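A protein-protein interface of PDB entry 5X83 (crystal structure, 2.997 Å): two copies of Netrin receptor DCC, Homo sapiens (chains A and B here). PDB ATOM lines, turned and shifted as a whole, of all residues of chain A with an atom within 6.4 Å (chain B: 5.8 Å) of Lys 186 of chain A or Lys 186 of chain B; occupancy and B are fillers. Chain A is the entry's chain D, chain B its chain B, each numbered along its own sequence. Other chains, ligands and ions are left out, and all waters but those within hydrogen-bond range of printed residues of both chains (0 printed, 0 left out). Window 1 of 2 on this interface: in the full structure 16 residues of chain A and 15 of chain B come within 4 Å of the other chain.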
ATOM      1  N   LEU A  13      15.123  -6.872  -4.512  1.00  0.00           N
ATOM      2  CA  LEU A  13      14.644  -5.498  -4.387  1.00  0.00           C
ATOM      3  C   LEU A  13      13.145  -5.414  -4.654  1.00  0.00           C
ATOM      4  O   LEU A  13      12.338  -5.513  -3.732  1.00  0.00           O
ATOM      5  CB  LEU A  13      15.398  -4.575  -5.341  1.00  0.00           C
ATOM      6  CG  LEU A  13      16.918  -4.587  -5.182  1.00  0.00           C
ATOM      7  CD1 LEU A  13      17.574  -3.690  -6.217  1.00  0.00           C
ATOM      8  CD2 LEU A  13      17.296  -4.161  -3.775  1.00  0.00           C
ATOM      9  N   TYR A  98      10.255 -10.724  -5.146  1.00  0.00           N
ATOM     10  CA  TYR A  98       9.016 -10.417  -4.438  1.00  0.00           C
ATOM     11  C   TYR A  98       7.793 -10.882  -5.212  1.00  0.00           C
ATOM     12  O   TYR A  98       7.890 -11.275  -6.374  1.00  0.00           O
ATOM     13  CB  TYR A  98       8.892  -8.910  -4.190  1.00  0.00           C
ATOM     14  CG  TYR A  98       9.774  -8.351  -3.095  1.00  0.00           C
ATOM     15  CD1 TYR A  98      10.788  -9.112  -2.527  1.00  0.00           C
ATOM     16  CD2 TYR A  98       9.588  -7.056  -2.629  1.00  0.00           C
ATOM     17  CE1 TYR A  98      11.595  -8.595  -1.530  1.00  0.00           C
ATOM     18  CE2 TYR A  98      10.383  -6.534  -1.631  1.00  0.00           C
ATOM     19  CZ  TYR A  98      11.387  -7.306  -1.086  1.00  0.00           C
ATOM     20  OH  TYR A  98      12.184  -6.786  -0.091  1.00  0.00           O
ATOM     21  N   GLU A  99       6.638 -10.829  -4.556  1.00  0.00           N
ATOM     22  CA  GLU A  99       5.390 -11.257  -5.173  1.00  0.00           C
ATOM     23  C   GLU A  99       4.753 -10.119  -5.952  1.00  0.00           C
ATOM     24  O   GLU A  99       5.107  -8.953  -5.774  1.00  0.00           O
ATOM     25  CB  GLU A  99       4.411 -11.783  -4.123  1.00  0.00           C
ATOM     26  CG  GLU A  99       4.684 -13.209  -3.678  1.00  0.00           C
ATOM     27  CD  GLU A  99       3.620 -13.734  -2.735  1.00  0.00           C
ATOM     28  OE1 GLU A  99       2.678 -12.977  -2.418  1.00  0.00           O
ATOM     29  OE2 GLU A  99       3.722 -14.905  -2.312  1.00  0.00           O
ATOM     30  N   ALA A 100       3.804 -10.465  -6.811  1.00  0.00           N
ATOM     31  CA  ALA A 100       3.084  -9.476  -7.595  1.00  0.00           C
ATOM     32  C   ALA A 100       1.646  -9.923  -7.791  1.00  0.00           C
ATOM     33  O   ALA A 100       1.339 -11.110  -7.685  1.00  0.00           O
ATOM     34  CB  ALA A 100       3.763  -9.256  -8.936  1.00  0.00           C
ATOM     35  N   ALA A 101       0.766  -8.966  -8.068  1.00  0.00           N
ATOM     36  CA  ALA A 101      -0.633  -9.270  -8.333  1.00  0.00           C
ATOM     37  C   ALA A 101      -0.739 -10.244  -9.501  1.00  0.00           C
ATOM     38  O   ALA A 101       0.069 -10.189 -10.429  1.00  0.00           O
ATOM     39  CB  ALA A 101      -1.411  -7.996  -8.624  1.00  0.00           C
ATOM     40  N   THR A 136      -4.068 -15.997  -2.017  1.00  0.00           N
ATOM     41  CA  THR A 136      -4.601 -15.894  -0.664  1.00  0.00           C
ATOM     42  C   THR A 136      -6.086 -16.224  -0.637  1.00  0.00           C
ATOM     43  O   THR A 136      -6.563 -16.921   0.260  1.00  0.00           O
ATOM     44  CB  THR A 136      -4.393 -14.485  -0.078  1.00  0.00           C
ATOM     45  OG1 THR A 136      -5.086 -13.520  -0.879  1.00  0.00           O
ATOM     46  CG2 THR A 136      -2.916 -14.137  -0.036  1.00  0.00           C
ATOM     47  N   ASN A 184      -4.226 -12.107  -3.867  1.00  0.00           N
ATOM     48  CA  ASN A 184      -2.819 -12.322  -3.577  1.00  0.00           C
ATOM     49  C   ASN A 184      -2.383 -11.292  -2.537  1.00  0.00           C
ATOM     50  O   ASN A 184      -3.031 -10.254  -2.391  1.00  0.00           O
ATOM     51  CB  ASN A 184      -1.994 -12.217  -4.863  1.00  0.00           C
ATOM     52  CG  ASN A 184      -0.510 -12.153  -4.607  1.00  0.00           C
ATOM     53  OD1 ASN A 184       0.089 -11.079  -4.634  1.00  0.00           O
ATOM     54  ND2 ASN A 184       0.095 -13.308  -4.354  1.00  0.00           N
ATOM     55  N   SER A 185      -1.308 -11.585  -1.807  1.00  0.00           N
ATOM     56  CA  SER A 185      -0.818 -10.715  -0.734  1.00  0.00           C
ATOM     57  C   SER A 185      -0.644  -9.237  -1.118  1.00  0.00           C
ATOM     58  O   SER A 185      -0.707  -8.362  -0.255  1.00  0.00           O
ATOM     59  CB  SER A 185       0.510 -11.259  -0.201  1.00  0.00           C
ATOM     60  OG  SER A 185       1.547 -11.103  -1.153  1.00  0.00           O
ATOM     61  N   LYS A 186      -0.428  -8.960  -2.403  1.00  0.00           N
ATOM     62  CA  LYS A 186      -0.206  -7.590  -2.865  1.00  0.00           C
ATOM     63  C   LYS A 186      -1.323  -7.046  -3.752  1.00  0.00           C
ATOM     64  O   LYS A 186      -1.235  -5.924  -4.253  1.00  0.00           O
ATOM     65  CB  LYS A 186       1.135  -7.492  -3.596  1.00  0.00           C
ATOM     66  CG  LYS A 186       2.323  -7.571  -2.657  1.00  0.00           C
ATOM     67  CD  LYS A 186       2.161  -6.538  -1.547  1.00  0.00           C
ATOM     68  CE  LYS A 186       3.065  -6.818  -0.365  1.00  0.00           C
ATOM     69  NZ  LYS A 186       2.553  -7.952   0.454  1.00  0.00           N
ATOM     70  N   GLY A 187      -2.375  -7.833  -3.937  1.00  0.00           N
ATOM     71  CA  GLY A 187      -3.514  -7.375  -4.709  1.00  0.00           C
ATOM     72  C   GLY A 187      -4.322  -8.483  -5.350  1.00  0.00           C
ATOM     73  O   GLY A 187      -4.118  -9.665  -5.074  1.00  0.00           O
ATOM     74  N   VAL A 188      -5.248  -8.090  -6.216  1.00  0.00           N
ATOM     75  CA  VAL A 188      -6.145  -9.034  -6.863  1.00  0.00           C
ATOM     76  C   VAL A 188      -6.028  -8.963  -8.387  1.00  0.00           C
ATOM     77  O   VAL A 188      -6.035  -7.881  -8.975  1.00  0.00           O
ATOM     78  CB  VAL A 188      -7.610  -8.796  -6.422  1.00  0.00           C
ATOM     79  CG1 VAL A 188      -8.001  -7.333  -6.584  1.00  0.00           C
ATOM     80  CG2 VAL A 188      -8.559  -9.719  -7.170  1.00  0.00           C
ATOM     81  N   HIS B  15      -2.071  -7.124   4.220  1.00  0.00           N
ATOM     82  CA  HIS B  15      -1.315  -7.153   5.464  1.00  0.00           C
ATOM     83  C   HIS B  15      -2.083  -6.462   6.586  1.00  0.00           C
ATOM     84  O   HIS B  15      -1.654  -6.466   7.738  1.00  0.00           O
ATOM     85  CB  HIS B  15       0.053  -6.492   5.279  1.00  0.00           C
ATOM     86  CG  HIS B  15      -0.015  -5.011   5.071  1.00  0.00           C
ATOM     87  ND1 HIS B  15      -0.169  -4.438   3.826  1.00  0.00           N
ATOM     88  CD2 HIS B  15       0.054  -3.982   5.951  1.00  0.00           C
ATOM     89  CE1 HIS B  15      -0.193  -3.123   3.948  1.00  0.00           C
ATOM     90  NE2 HIS B  15      -0.059  -2.821   5.227  1.00  0.00           N
ATOM     91  N   TYR B  98      -0.687 -10.999   6.518  1.00  0.00           N
ATOM     92  CA  TYR B  98       0.572 -11.123   5.799  1.00  0.00           C
ATOM     93  C   TYR B  98       1.595 -10.073   6.230  1.00  0.00           C
ATOM     94  O   TYR B  98       1.286  -9.165   7.001  1.00  0.00           O
ATOM     95  CB  TYR B  98       0.321 -11.067   4.293  1.00  0.00           C
ATOM     96  CG  TYR B  98      -0.222 -12.374   3.764  1.00  0.00           C
ATOM     97  CD1 TYR B  98      -1.567 -12.696   3.891  1.00  0.00           C
ATOM     98  CD2 TYR B  98       0.620 -13.303   3.163  1.00  0.00           C
ATOM     99  CE1 TYR B  98      -2.061 -13.900   3.420  1.00  0.00           C
ATOM    100  CE2 TYR B  98       0.136 -14.507   2.689  1.00  0.00           C
ATOM    101  CZ  TYR B  98      -1.204 -14.802   2.821  1.00  0.00           C
ATOM    102  OH  TYR B  98      -1.686 -16.001   2.348  1.00  0.00           O
ATOM    103  N   GLU B  99       2.814 -10.202   5.716  1.00  0.00           N
ATOM    104  CA  GLU B  99       3.900  -9.314   6.102  1.00  0.00           C
ATOM    105  C   GLU B  99       3.874  -8.012   5.313  1.00  0.00           C
ATOM    106  O   GLU B  99       3.212  -7.909   4.282  1.00  0.00           O
ATOM    107  CB  GLU B  99       5.243 -10.015   5.900  1.00  0.00           C
ATOM    108  CG  GLU B  99       5.602 -10.999   6.998  1.00  0.00           C
ATOM    109  CD  GLU B  99       6.985 -11.595   6.814  1.00  0.00           C
ATOM    110  OE1 GLU B  99       7.400 -12.412   7.664  1.00  0.00           O
ATOM    111  OE2 GLU B  99       7.655 -11.251   5.818  1.00  0.00           O
ATOM    112  N   ALA B 100       4.597  -7.017   5.817  1.00  0.00           N
ATOM    113  CA  ALA B 100       4.701  -5.720   5.160  1.00  0.00           C
ATOM    114  C   ALA B 100       6.087  -5.135   5.397  1.00  0.00           C
ATOM    115  O   ALA B 100       6.772  -5.525   6.341  1.00  0.00           O
ATOM    116  CB  ALA B 100       3.623  -4.775   5.666  1.00  0.00           C
ATOM    117  N   ALA B 101       6.500  -4.213   4.534  1.00  0.00           N
ATOM    118  CA  ALA B 101       7.792  -3.548   4.687  1.00  0.00           C
ATOM    119  C   ALA B 101       7.895  -2.839   6.035  1.00  0.00           C
ATOM    120  O   ALA B 101       6.909  -2.287   6.525  1.00  0.00           O
ATOM    121  CB  ALA B 101       8.014  -2.561   3.552  1.00  0.00           C
ATOM    122  N   ASN B 184      13.233  -6.660   3.980  1.00  0.00           N
ATOM    123  CA  ASN B 184      12.211  -7.621   4.353  1.00  0.00           C
ATOM    124  C   ASN B 184      11.552  -8.164   3.093  1.00  0.00           C
ATOM    125  O   ASN B 184      11.608  -7.527   2.042  1.00  0.00           O
ATOM    126  CB  ASN B 184      11.187  -6.957   5.280  1.00  0.00           C
ATOM    127  CG  ASN B 184       9.944  -7.790   5.483  1.00  0.00           C
ATOM    128  OD1 ASN B 184       8.912  -7.544   4.859  1.00  0.00           O
ATOM    129  ND2 ASN B 184      10.034  -8.786   6.356  1.00  0.00           N
ATOM    130  N   SER B 185      10.946  -9.344   3.195  1.00  0.00           N
ATOM    131  CA  SER B 185      10.302 -10.001   2.061  1.00  0.00           C
ATOM    132  C   SER B 185       9.342  -9.093   1.287  1.00  0.00           C
ATOM    133  O   SER B 185       9.065  -9.341   0.115  1.00  0.00           O
ATOM    134  CB  SER B 185       9.549 -11.248   2.530  1.00  0.00           C
ATOM    135  OG  SER B 185       8.404 -10.900   3.287  1.00  0.00           O
ATOM    136  N   LYS B 186       8.824  -8.054   1.940  1.00  0.00           N
ATOM    137  CA  LYS B 186       7.845  -7.182   1.298  1.00  0.00           C
ATOM    138  C   LYS B 186       8.349  -5.757   1.040  1.00  0.00           C
ATOM    139  O   LYS B 186       7.605  -4.917   0.532  1.00  0.00           O
ATOM    140  CB  LYS B 186       6.573  -7.124   2.147  1.00  0.00           C
ATOM    141  CG  LYS B 186       5.818  -8.443   2.201  1.00  0.00           C
ATOM    142  CD  LYS B 186       5.593  -9.020   0.816  1.00  0.00           C
ATOM    143  CE  LYS B 186       5.216 -10.491   0.893  1.00  0.00           C
ATOM    144  NZ  LYS B 186       4.058 -10.718   1.803  1.00  0.00           N
ATOM    145  N   GLY B 187       9.606  -5.482   1.377  1.00  0.00           N
ATOM    146  CA  GLY B 187      10.180  -4.173   1.117  1.00  0.00           C
ATOM    147  C   GLY B 187      11.304  -3.772   2.056  1.00  0.00           C
ATOM    148  O   GLY B 187      11.794  -4.587   2.838  1.00  0.00           O
ATOM    149  N   VAL B 188      11.717  -2.510   1.977  1.00  0.00           N
ATOM    150  CA  VAL B 188      12.825  -2.014   2.788  1.00  0.00           C
ATOM    151  C   VAL B 188      12.419  -0.831   3.664  1.00  0.00           C
ATOM    152  O   VAL B 188      11.809   0.129   3.194  1.00  0.00           O
ATOM    153  CB  VAL B 188      14.028  -1.605   1.897  1.00  0.00           C
ATOM    154  CG1 VAL B 188      13.593  -0.648   0.793  1.00  0.00           C
ATOM    155  CG2 VAL B 188      15.150  -1.005   2.738  1.00  0.00           C
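The side-chain hydroxyl (OH) of Tyr 98 of chain A lies within hydrogen-bond range of the backbone NH (N) of Gly 187 of chain B. The backbone carbonyl oxygen (O) of Asn 184 of chain B lies close to the side-chain hydroxyl (OH) of Tyr 98 of chain A, 2.3 Å away. The side-chain amino group of Lys 186 of chain A lies close to the side-chain amino group of Lys 186 of chain B (3.4 Å).
The side-chain amide oxygen (OD1) of Asn 184 of chain B lies close to the backbone carbonyl oxygen (O) of Ala 100 of chain B, 3.3 Å away. The side-chain hydroxyl (OG) of Ser 185 of chain B is in hydrogen-bond range of the side-chain carboxylate (OE2) of Glu 99 of chain B (2.7 Å). The side-chain carboxylate (OE1) of Glu 99 of chain A sits at hydrogen-bond distance from the side-chain hydroxyl (OG) of Ser 185 of chain A (2.5 Å). The side-chain amide oxygen (OD1) of Asn 184 of chain B lies close to the backbone NH (N) of Lys 186 of chain B (3.0 Å). ND2 of Asn 184 of chain B is in hydrogen-bond range of OE2 of Glu 99 of chain B. N of Lys 186 of chain A lies close to OD1 of Asn 184 of chain A, at 3.1 Å.
Ser 185 of chain B touches Tyr 98 of chain A. Tyr 98 of chain A touches Lys 186 of chain B. Tyr 98 of chain B touches Thr 136 of chain A (OH to CG2, 3.3 Å). CD2 of Tyr 98 of chain B touches CB of Ser 185 of chain A, at 3.9 Å. Lys 186 of chain B touches Ser 185 of chain A. O of Glu 99 of chain B touches NZ of Lys 186 of chain A, at 3.9 Å.
Of the printed residues of chain B, Ser 185 of chain A touches Tyr 98 and Lys 186. Lys 186 of chain A touches two residues of chain B. Gly 187 of chain A touches none of the printed residues of chain B. Of chain A, only Tyr 98, Ser 185 and Lys 186 come within 4 Å of Lys 186 of chain B. Of the printed residues of chain A, Gly 187 of chain B touches Tyr 98 (3.2 Å). The nearest residue of chain A that does not touch Lys 186 of chain B is Glu 99 of chain A (4.9 Å). The nearest printed residue of chain B that does not touch Ser 185 of chain A is His 15 of chain B (4.8 Å).
Hydrophobic or aromatic side chains of chain B within 4 Å of the printed part of chain A: Tyr 98. Of the 11 printed residues of chain A, 4 touch a printed residue of chain B. Printed residues of chain A that touch a printed residue of chain B: Tyr 98, Thr 136, Ser 185 and Lys 186. Among the printed residues, 9 pairs touch across the chains.
Tyr 98 of chain A touches Asn 184 of chain B, but with the chains exchanged Asn 184 of chain A does not touch Tyr 98 of chain B (6.5 Å). Tyr 98 of chain A touches Ser 185 of chain B, and with the chains exchanged Ser 185 of chain A touches Tyr 98 of chain B. Tyr 98 of chain A touches Lys 186 of chain B, but with the chains exchanged Lys 186 of chain A does not touch Tyr 98 of chain B (5.4 Å). Tyr 98 of chain A touches Gly 187 of chain B, but with the chains exchanged Gly 187 of chain A does not touch Tyr 98 of chain B (9.2 Å). Positions printed for both chains: 98, 99, 100, 101, 184, 185, 186, 187 and 188. Of the 9 pairs that touch across the chains among the printed residues, 3 have their exchanged pair printed and touching as well.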
